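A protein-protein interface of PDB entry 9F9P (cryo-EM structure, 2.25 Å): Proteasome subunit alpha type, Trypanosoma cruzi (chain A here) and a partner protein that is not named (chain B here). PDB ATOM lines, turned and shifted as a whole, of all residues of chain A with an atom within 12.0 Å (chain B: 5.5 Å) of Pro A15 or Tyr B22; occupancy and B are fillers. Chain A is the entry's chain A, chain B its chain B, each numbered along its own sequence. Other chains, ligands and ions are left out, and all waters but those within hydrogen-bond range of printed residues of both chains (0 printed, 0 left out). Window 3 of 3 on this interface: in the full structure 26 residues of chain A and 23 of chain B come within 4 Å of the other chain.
The backbone carbonyl oxygen (O) of Phe A13 is in hydrogen-bond range of the side-chain amide nitrogen (NE2) of Gln B19, at 3.0 Å.
The side-chain hydroxyl (OG) of Ser A14 sits close to the backbone NH (N) of Glu A16 (3.5 Å). The side-chain hydroxyl (OG) of Ser A14 sits at hydrogen-bond distance from the side-chain hydroxyl (OG) of Ser A18 (2.9 Å). The backbone carbonyl oxygen (O) of Glu B21 lies within hydrogen-bond range of the side-chain hydroxyl (OG1) of Thr B25, at 3.5 Å.
Among the printed residues, merely in contact across the chains: Gly A17 with Ala B26 (3.4 Å), Phe A13 with Ala B23 (3.5 Å), Ser A14 with Tyr B22 (3.6 Å), Val A12 with Gln B19 (3.6 Å), Phe A13 with Tyr B22 (3.7 Å), Pro A15 with Tyr B22 (3.8 Å), Gly A17 with Tyr B22 (3.8 Å) and Glu A16 with Thr B25 (3.8 Å).
Tyr B22 touches just these residues of chain A: Phe A13 (3.7 Å), Ser A14 (3.6 Å), Pro A15 (3.8 Å) and Gly A17 (3.8 Å). No residue of chain A comes within 4 Å of Val B18. Of chain A, only Val A12 (3.6 Å) and Phe A13 (3.0 Å) come within 4 Å of Gln B19. No residue of chain A comes within 4 Å of Glu B21. Of chain A, only Glu A16 comes within 4 Å of Thr B25. Ala B26 touches one residue of chain A. Of the printed residues of chain B, Phe A13 touches Gln B19, Tyr B22 and Ala B23. Of the printed residues of chain B, Val A12 touches Gln B19. Printed residues of chain B within 4 Å of Ser A14: Tyr B22. Of the printed residues of chain B, Glu A16 touches Thr B25 (3.8 Å). Of the printed residues of chain B, Gly A17 touches Tyr B22 (3.8 Å) and Ala B26 (3.4 Å). Phe A6 touches none of the printed residues of chain B. The nearest residue of chain A that does not touch Tyr B22 is Glu A16 (5.4 Å).
Printed residues of chain B that touch a printed residue of chain A: Gln B19, Tyr B22, Ala B23, Thr B25 and Ala B26. Hydrophobic or aromatic side chains of chain B within 4 Å of the printed part of chain A: Tyr B22, Ala B23 and Ala B26. Along chain A the printed residues that touch a printed residue of chain B span positions 12 to 17. Among the printed residues, no Asp or Glu carboxylate lies within 4 Å of a Lys or Arg side-chain nitrogen of the other chain.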
ATOM      1  N   PHE A   6     -13.210  24.403  27.445  1.00  0.00           N
ATOM      2  CA  PHE A   6     -13.756  25.733  27.041  1.00  0.00           C
ATOM      3  C   PHE A   6     -14.882  26.123  28.005  1.00  0.00           C
ATOM      4  O   PHE A   6     -14.861  27.185  28.615  1.00  0.00           O
ATOM      5  CB  PHE A   6     -14.175  25.644  25.577  1.00  0.00           C
ATOM      6  CG  PHE A   6     -14.157  26.923  24.783  1.00  0.00           C
ATOM      7  CD1 PHE A   6     -13.133  27.171  23.867  1.00  0.00           C
ATOM      8  CD2 PHE A   6     -15.227  27.807  24.840  1.00  0.00           C
ATOM      9  CE1 PHE A   6     -13.151  28.302  23.061  1.00  0.00           C
ATOM     10  CE2 PHE A   6     -15.245  28.940  24.034  1.00  0.00           C
ATOM     11  CZ  PHE A   6     -14.207  29.187  23.149  1.00  0.00           C
ATOM     12  N   ASP A   7     -15.837  25.216  28.163  1.00  0.00           N
ATOM     13  CA  ASP A   7     -16.742  25.194  29.296  1.00  0.00           C
ATOM     14  C   ASP A   7     -16.001  25.021  30.636  1.00  0.00           C
ATOM     15  O   ASP A   7     -16.532  25.377  31.689  1.00  0.00           O
ATOM     16  CB  ASP A   7     -17.786  24.078  29.135  1.00  0.00           C
ATOM     17  CG  ASP A   7     -17.238  22.698  28.808  1.00  0.00           C
ATOM     18  OD1 ASP A   7     -16.100  22.612  28.303  1.00  0.00           O
ATOM     19  OD2 ASP A   7     -17.947  21.719  29.062  1.00  0.00           O
ATOM     20  N   LYS A   8     -14.771  24.499  30.609  1.00  0.00           N
ATOM     21  CA  LYS A   8     -13.957  24.411  31.809  1.00  0.00           C
ATOM     22  C   LYS A   8     -13.353  25.747  32.216  1.00  0.00           C
ATOM     23  O   LYS A   8     -13.015  25.883  33.384  1.00  0.00           O
ATOM     24  CB  LYS A   8     -12.880  23.348  31.656  1.00  0.00           C
ATOM     25  CG  LYS A   8     -13.472  22.010  31.285  1.00  0.00           C
ATOM     26  CD  LYS A   8     -13.207  20.899  32.257  1.00  0.00           C
ATOM     27  CE  LYS A   8     -14.017  19.664  31.905  1.00  0.00           C
ATOM     28  NZ  LYS A   8     -13.602  19.100  30.592  1.00  0.00           N
ATOM     29  N   TYR A   9     -13.273  26.730  31.319  1.00  0.00           N
ATOM     30  CA  TYR A   9     -12.484  27.925  31.589  1.00  0.00           C
ATOM     31  C   TYR A   9     -13.356  29.162  31.760  1.00  0.00           C
ATOM     32  O   TYR A   9     -12.975  30.040  32.514  1.00  0.00           O
ATOM     33  CB  TYR A   9     -11.398  28.123  30.516  1.00  0.00           C
ATOM     34  CG  TYR A   9     -10.541  26.892  30.331  1.00  0.00           C
ATOM     35  CD1 TYR A   9      -9.995  26.252  31.439  1.00  0.00           C
ATOM     36  CD2 TYR A   9     -10.331  26.316  29.080  1.00  0.00           C
ATOM     37  CE1 TYR A   9      -9.265  25.085  31.319  1.00  0.00           C
ATOM     38  CE2 TYR A   9      -9.546  25.172  28.939  1.00  0.00           C
ATOM     39  CZ  TYR A   9      -9.022  24.549  30.066  1.00  0.00           C
ATOM     40  OH  TYR A   9      -8.281  23.385  30.022  1.00  0.00           O
ATOM     41  N   ILE A  10     -14.521  29.241  31.112  1.00  0.00           N
ATOM     42  CA  ILE A  10     -15.395  30.389  31.301  1.00  0.00           C
ATOM     43  C   ILE A  10     -16.794  29.939  31.706  1.00  0.00           C
ATOM     44  O   ILE A  10     -17.089  28.750  31.702  1.00  0.00           O
ATOM     45  CB  ILE A  10     -15.417  31.265  30.035  1.00  0.00           C
ATOM     46  CG1 ILE A  10     -15.607  30.435  28.772  1.00  0.00           C
ATOM     47  CG2 ILE A  10     -14.159  32.117  29.945  1.00  0.00           C
ATOM     48  CD1 ILE A  10     -15.999  31.264  27.584  1.00  0.00           C
ATOM     49  N   THR A  11     -17.634  30.911  32.071  1.00  0.00           N
ATOM     50  CA  THR A  11     -19.033  30.661  32.388  1.00  0.00           C
ATOM     51  C   THR A  11     -19.857  30.532  31.103  1.00  0.00           C
ATOM     52  O   THR A  11     -20.355  31.512  30.587  1.00  0.00           O
ATOM     53  CB  THR A  11     -19.620  31.739  33.327  1.00  0.00           C
ATOM     54  OG1 THR A  11     -19.373  33.071  32.842  1.00  0.00           O
ATOM     55  CG2 THR A  11     -19.121  31.579  34.757  1.00  0.00           C
ATOM     56  N   VAL A  12     -19.898  29.316  30.558  1.00  0.00           N
ATOM     57  CA  VAL A  12     -20.882  28.875  29.597  1.00  0.00           C
ATOM     58  C   VAL A  12     -21.333  27.509  30.063  1.00  0.00           C
ATOM     59  O   VAL A  12     -20.632  26.899  30.843  1.00  0.00           O
ATOM     60  CB  VAL A  12     -20.309  28.789  28.162  1.00  0.00           C
ATOM     61  CG1 VAL A  12     -19.891  30.151  27.652  1.00  0.00           C
ATOM     62  CG2 VAL A  12     -19.163  27.804  28.049  1.00  0.00           C
ATOM     63  N   PHE A  13     -22.440  27.012  29.520  1.00  0.00           N
ATOM     64  CA  PHE A  13     -22.932  25.695  29.873  1.00  0.00           C
ATOM     65  C   PHE A  13     -22.134  24.599  29.208  1.00  0.00           C
ATOM     66  O   PHE A  13     -21.664  24.752  28.110  1.00  0.00           O
ATOM     67  CB  PHE A  13     -24.381  25.482  29.456  1.00  0.00           C
ATOM     68  CG  PHE A  13     -25.368  26.279  30.251  1.00  0.00           C
ATOM     69  CD1 PHE A  13     -25.721  25.889  31.517  1.00  0.00           C
ATOM     70  CD2 PHE A  13     -25.940  27.427  29.725  1.00  0.00           C
ATOM     71  CE1 PHE A  13     -26.600  26.658  32.275  1.00  0.00           C
ATOM     72  CE2 PHE A  13     -26.835  28.177  30.476  1.00  0.00           C
ATOM     73  CZ  PHE A  13     -27.184  27.783  31.746  1.00  0.00           C
ATOM     74  N   SER A  14     -21.946  23.514  29.945  1.00  0.00           N
ATOM     75  CA  SER A  14     -21.486  22.244  29.409  1.00  0.00           C
ATOM     76  C   SER A  14     -22.677  21.560  28.756  1.00  0.00           C
ATOM     77  O   SER A  14     -23.804  21.986  28.975  1.00  0.00           O
ATOM     78  CB  SER A  14     -20.943  21.380  30.515  1.00  0.00           C
ATOM     79  OG  SER A  14     -22.017  20.878  31.331  1.00  0.00           O
ATOM     80  N   PRO A  15     -22.498  20.484  27.975  1.00  0.00           N
ATOM     81  CA  PRO A  15     -23.639  19.732  27.423  1.00  0.00           C
ATOM     82  C   PRO A  15     -24.659  19.084  28.358  1.00  0.00           C
ATOM     83  O   PRO A  15     -25.764  18.760  27.931  1.00  0.00           O
ATOM     84  CB  PRO A  15     -22.976  18.591  26.635  1.00  0.00           C
ATOM     85  CG  PRO A  15     -21.613  19.171  26.267  1.00  0.00           C
ATOM     86  CD  PRO A  15     -21.206  20.043  27.442  1.00  0.00           C
ATOM     87  N   GLU A  16     -24.303  18.875  29.620  1.00  0.00           N
ATOM     88  CA  GLU A  16     -25.206  18.282  30.596  1.00  0.00           C
ATOM     89  C   GLU A  16     -25.953  19.364  31.368  1.00  0.00           C
ATOM     90  O   GLU A  16     -26.641  19.049  32.329  1.00  0.00           O
ATOM     91  CB  GLU A  16     -24.412  17.461  31.616  1.00  0.00           C
ATOM     92  CG  GLU A  16     -23.708  16.248  31.012  1.00  0.00           C
ATOM     93  CD  GLU A  16     -22.555  16.500  30.042  1.00  0.00           C
ATOM     94  OE1 GLU A  16     -22.180  15.546  29.320  1.00  0.00           O
ATOM     95  OE2 GLU A  16     -22.011  17.637  30.016  1.00  0.00           O
ATOM     96  N   GLY A  17     -25.750  20.640  31.025  1.00  0.00           N
ATOM     97  CA  GLY A  17     -26.469  21.720  31.683  1.00  0.00           C
ATOM     98  C   GLY A  17     -25.764  22.334  32.901  1.00  0.00           C
ATOM     99  O   GLY A  17     -26.372  23.139  33.603  1.00  0.00           O
ATOM    100  N   SER A  18     -24.480  22.048  33.124  1.00  0.00           N
ATOM    101  CA  SER A  18     -23.814  22.468  34.354  1.00  0.00           C
ATOM    102  C   SER A  18     -22.841  23.610  34.080  1.00  0.00           C
ATOM    103  O   SER A  18     -22.589  23.908  32.915  1.00  0.00           O
ATOM    104  CB  SER A  18     -23.110  21.283  34.992  1.00  0.00           C
ATOM    105  OG  SER A  18     -21.936  20.954  34.264  1.00  0.00           O
ATOM    106  N   LEU A  19     -22.325  24.235  35.155  1.00  0.00           N
ATOM    107  CA  LEU A  19     -21.313  25.281  35.087  1.00  0.00           C
ATOM    108  C   LEU A  19     -20.083  24.896  35.905  1.00  0.00           C
ATOM    109  O   LEU A  19     -20.113  24.899  37.129  1.00  0.00           O
ATOM    110  CB  LEU A  19     -21.919  26.581  35.620  1.00  0.00           C
ATOM    111  CG  LEU A  19     -23.201  27.071  34.924  1.00  0.00           C
ATOM    112  CD1 LEU A  19     -24.012  28.022  35.825  1.00  0.00           C
ATOM    113  CD2 LEU A  19     -22.861  27.807  33.634  1.00  0.00           C
ATOM    114  N   TYR A  20     -18.965  24.613  35.232  1.00  0.00           N
ATOM    115  CA  TYR A  20     -17.797  24.041  35.878  1.00  0.00           C
ATOM    116  C   TYR A  20     -17.067  25.080  36.712  1.00  0.00           C
ATOM    117  O   TYR A  20     -16.598  24.761  37.788  1.00  0.00           O
ATOM    118  CB  TYR A  20     -16.864  23.413  34.853  1.00  0.00           C
ATOM    119  CG  TYR A  20     -17.309  22.077  34.319  1.00  0.00           C
ATOM    120  CD1 TYR A  20     -17.460  20.975  35.147  1.00  0.00           C
ATOM    121  CD2 TYR A  20     -17.517  21.891  32.962  1.00  0.00           C
ATOM    122  CE1 TYR A  20     -17.856  19.743  34.649  1.00  0.00           C
ATOM    123  CE2 TYR A  20     -17.910  20.665  32.448  1.00  0.00           C
ATOM    124  CZ  TYR A  20     -18.091  19.593  33.295  1.00  0.00           C
ATOM    125  OH  TYR A  20     -18.470  18.400  32.743  1.00  0.00           O
ATOM    126  N   GLN A  21     -16.994  26.333  36.287  1.00  0.00           N
ATOM    127  CA  GLN A  21     -16.318  27.279  37.148  1.00  0.00           C
ATOM    128  C   GLN A  21     -17.067  27.388  38.486  1.00  0.00           C
ATOM    129  O   GLN A  21     -16.436  27.676  39.499  1.00  0.00           O
ATOM    130  CB  GLN A  21     -16.122  28.649  36.478  1.00  0.00           C
ATOM    131  CG  GLN A  21     -14.919  28.732  35.538  1.00  0.00           C
ATOM    132  CD  GLN A  21     -13.622  28.584  36.300  1.00  0.00           C
ATOM    133  OE1 GLN A  21     -13.361  29.323  37.250  1.00  0.00           O
ATOM    134  NE2 GLN A  21     -12.795  27.645  35.878  1.00  0.00           N
ATOM    135  N   GLU A  23     -18.677  24.761  40.063  1.00  0.00           N
ATOM    136  CA  GLU A  23     -18.242  23.602  40.832  1.00  0.00           C
ATOM    137  C   GLU A  23     -16.852  23.775  41.459  1.00  0.00           C
ATOM    138  O   GLU A  23     -16.587  23.217  42.502  1.00  0.00           O
ATOM    139  CB  GLU A  23     -18.135  22.357  39.969  1.00  0.00           C
ATOM    140  CG  GLU A  23     -19.461  21.815  39.505  1.00  0.00           C
ATOM    141  CD  GLU A  23     -19.289  20.587  38.616  1.00  0.00           C
ATOM    142  OE1 GLU A  23     -18.397  19.735  38.951  1.00  0.00           O
ATOM    143  OE2 GLU A  23     -20.014  20.493  37.572  1.00  0.00           O
ATOM    144  N   TYR A  24     -15.940  24.424  40.755  1.00  0.00           N
ATOM    145  CA  TYR A  24     -14.552  24.507  41.152  1.00  0.00           C
ATOM    146  C   TYR A  24     -14.344  25.561  42.230  1.00  0.00           C
ATOM    147  O   TYR A  24     -13.541  25.380  43.131  1.00  0.00           O
ATOM    148  CB  TYR A  24     -13.692  24.895  39.951  1.00  0.00           C
ATOM    149  CG  TYR A  24     -13.571  23.871  38.841  1.00  0.00           C
ATOM    150  CD1 TYR A  24     -14.046  22.570  38.966  1.00  0.00           C
ATOM    151  CD2 TYR A  24     -12.976  24.236  37.630  1.00  0.00           C
ATOM    152  CE1 TYR A  24     -13.948  21.663  37.917  1.00  0.00           C
ATOM    153  CE2 TYR A  24     -12.840  23.329  36.585  1.00  0.00           C
ATOM    154  CZ  TYR A  24     -13.310  22.032  36.741  1.00  0.00           C
ATOM    155  OH  TYR A  24     -13.164  21.166  35.691  1.00  0.00           O
ATOM    156  N   GLN A 124     -22.804  34.632  35.211  1.00  0.00           N
ATOM    157  CA  GLN A 124     -23.504  34.836  33.959  1.00  0.00           C
ATOM    158  C   GLN A 124     -22.748  35.803  33.060  1.00  0.00           C
ATOM    159  O   GLN A 124     -23.006  35.790  31.874  1.00  0.00           O
ATOM    160  CB  GLN A 124     -24.916  35.328  34.252  1.00  0.00           C
ATOM    161  CG  GLN A 124     -25.831  35.329  33.038  1.00  0.00           C
ATOM    162  CD  GLN A 124     -27.300  35.504  33.317  1.00  0.00           C
ATOM    163  OE1 GLN A 124     -27.711  36.064  34.335  1.00  0.00           O
ATOM    164  NE2 GLN A 124     -28.112  35.042  32.373  1.00  0.00           N
ATOM    165  N   ARG B  16     -27.697  25.107  14.354  1.00  0.00           N
ATOM    166  CA  ARG B  16     -28.122  24.993  15.739  1.00  0.00           C
ATOM    167  C   ARG B  16     -27.441  26.073  16.564  1.00  0.00           C
ATOM    168  O   ARG B  16     -26.345  26.486  16.232  1.00  0.00           O
ATOM    169  CB  ARG B  16     -27.742  23.610  16.259  1.00  0.00           C
ATOM    170  CG  ARG B  16     -28.670  22.498  15.791  1.00  0.00           C
ATOM    171  CD  ARG B  16     -28.085  21.109  16.032  1.00  0.00           C
ATOM    172  NE  ARG B  16     -28.020  20.674  17.430  1.00  0.00           N
ATOM    173  CZ  ARG B  16     -26.923  20.188  18.017  1.00  0.00           C
ATOM    174  NH1 ARG B  16     -25.780  20.112  17.350  1.00  0.00           N
ATOM    175  NH2 ARG B  16     -26.960  19.799  19.283  1.00  0.00           N
ATOM    176  N   VAL B  18     -26.116  25.947  20.142  1.00  0.00           N
ATOM    177  CA  VAL B  18     -26.037  24.880  21.135  1.00  0.00           C
ATOM    178  C   VAL B  18     -26.126  25.410  22.572  1.00  0.00           C
ATOM    179  O   VAL B  18     -26.733  24.775  23.419  1.00  0.00           O
ATOM    180  CB  VAL B  18     -24.856  23.904  20.972  1.00  0.00           C
ATOM    181  CG1 VAL B  18     -24.809  23.254  19.618  1.00  0.00           C
ATOM    182  CG2 VAL B  18     -23.535  24.539  21.289  1.00  0.00           C
ATOM    183  N   GLN B  19     -25.607  26.578  22.865  1.00  0.00           N
ATOM    184  CA  GLN B  19     -25.775  27.092  24.206  1.00  0.00           C
ATOM    185  C   GLN B  19     -27.236  27.270  24.602  1.00  0.00           C
ATOM    186  O   GLN B  19     -27.536  27.296  25.778  1.00  0.00           O
ATOM    187  CB  GLN B  19     -25.071  28.434  24.359  1.00  0.00           C
ATOM    188  CG  GLN B  19     -23.577  28.259  24.532  1.00  0.00           C
ATOM    189  CD  GLN B  19     -23.221  27.712  25.906  1.00  0.00           C
ATOM    190  OE1 GLN B  19     -23.634  28.244  26.933  1.00  0.00           O
ATOM    191  NE2 GLN B  19     -22.432  26.647  25.914  1.00  0.00           N
ATOM    192  N   ILE B  20     -28.150  27.429  23.647  1.00  0.00           N
ATOM    193  CA  ILE B  20     -29.542  27.567  24.008  1.00  0.00           C
ATOM    194  C   ILE B  20     -30.122  26.197  24.309  1.00  0.00           C
ATOM    195  O   ILE B  20     -30.881  26.081  25.264  1.00  0.00           O
ATOM    196  CB  ILE B  20     -30.334  28.345  22.951  1.00  0.00           C
ATOM    197  CG1 ILE B  20     -29.888  29.797  22.850  1.00  0.00           C
ATOM    198  CG2 ILE B  20     -31.813  28.353  23.234  1.00  0.00           C
ATOM    199  CD1 ILE B  20     -30.592  30.473  21.681  1.00  0.00           C
ATOM    200  N   GLU B  21     -29.691  25.160  23.598  1.00  0.00           N
ATOM    201  CA  GLU B  21     -30.071  23.803  23.954  1.00  0.00           C
ATOM    202  C   GLU B  21     -29.523  23.368  25.311  1.00  0.00           C
ATOM    203  O   GLU B  21     -30.190  22.675  26.047  1.00  0.00           O
ATOM    204  CB  GLU B  21     -29.540  22.797  22.948  1.00  0.00           C
ATOM    205  CG  GLU B  21     -29.886  23.168  21.525  1.00  0.00           C
ATOM    206  CD  GLU B  21     -29.419  22.149  20.497  1.00  0.00           C
ATOM    207  OE1 GLU B  21     -29.717  22.354  19.294  1.00  0.00           O
ATOM    208  OE2 GLU B  21     -28.744  21.151  20.903  1.00  0.00           O
ATOM    209  N   TYR B  22     -28.280  23.714  25.612  1.00  0.00           N
ATOM    210  CA  TYR B  22     -27.676  23.300  26.874  1.00  0.00           C
ATOM    211  C   TYR B  22     -28.366  23.994  28.028  1.00  0.00           C
ATOM    212  O   TYR B  22     -28.654  23.357  29.017  1.00  0.00           O
ATOM    213  CB  TYR B  22     -26.181  23.599  26.889  1.00  0.00           C
ATOM    214  CG  TYR B  22     -25.373  22.839  25.867  1.00  0.00           C
ATOM    215  CD1 TYR B  22     -25.921  21.777  25.178  1.00  0.00           C
ATOM    216  CD2 TYR B  22     -24.053  23.183  25.602  1.00  0.00           C
ATOM    217  CE1 TYR B  22     -25.190  21.086  24.226  1.00  0.00           C
ATOM    218  CE2 TYR B  22     -23.305  22.506  24.644  1.00  0.00           C
ATOM    219  CZ  TYR B  22     -23.886  21.457  23.945  1.00  0.00           C
ATOM    220  OH  TYR B  22     -23.209  20.763  22.964  1.00  0.00           O
ATOM    221  N   ALA B  23     -28.728  25.258  27.852  1.00  0.00           N
ATOM    222  CA  ALA B  23     -29.506  25.963  28.844  1.00  0.00           C
ATOM    223  C   ALA B  23     -30.880  25.368  29.007  1.00  0.00           C
ATOM    224  O   ALA B  23     -31.450  25.449  30.089  1.00  0.00           O
ATOM    225  CB  ALA B  23     -29.660  27.409  28.509  1.00  0.00           C
ATOM    226  N   THR B  24     -31.439  24.834  27.938  1.00  0.00           N
ATOM    227  CA  THR B  24     -32.751  24.229  28.009  1.00  0.00           C
ATOM    228  C   THR B  24     -32.680  22.868  28.689  1.00  0.00           C
ATOM    229  O   THR B  24     -33.647  22.467  29.304  1.00  0.00           O
ATOM    230  CB  THR B  24     -33.383  24.191  26.612  1.00  0.00           C
ATOM    231  OG1 THR B  24     -33.485  25.522  26.086  1.00  0.00           O
ATOM    232  CG2 THR B  24     -34.762  23.581  26.623  1.00  0.00           C
ATOM    233  N   THR B  25     -31.553  22.172  28.589  1.00  0.00           N
ATOM    234  CA  THR B  25     -31.323  20.939  29.325  1.00  0.00           C
ATOM    235  C   THR B  25     -31.221  21.211  30.832  1.00  0.00           C
ATOM    236  O   THR B  25     -31.737  20.457  31.623  1.00  0.00           O
ATOM    237  CB  THR B  25     -30.056  20.251  28.794  1.00  0.00           C
ATOM    238  OG1 THR B  25     -30.347  19.540  27.594  1.00  0.00           O
ATOM    239  CG2 THR B  25     -29.477  19.247  29.763  1.00  0.00           C
ATOM    240  N   ALA B  26     -30.583  22.317  31.233  1.00  0.00           N
ATOM    241  CA  ALA B  26     -30.518  22.706  32.638  1.00  0.00           C
ATOM    242  C   ALA B  26     -31.887  23.003  33.231  1.00  0.00           C
ATOM    243  O   ALA B  26     -32.119  22.686  34.388  1.00  0.00           O
ATOM    244  CB  ALA B  26     -29.628  23.913  32.806  1.00  0.00           C
ATOM    245  N   ALA B  27     -32.779  23.628  32.452  1.00  0.00           N
ATOM    246  CA  ALA B  27     -34.156  23.891  32.861  1.00  0.00           C
ATOM    247  C   ALA B  27     -34.947  22.609  33.021  1.00  0.00           C
ATOM    248  O   ALA B  27     -35.835  22.539  33.856  1.00  0.00           O
ATOM    249  CB  ALA B  27     -34.857  24.822  31.895  1.00  0.00           C
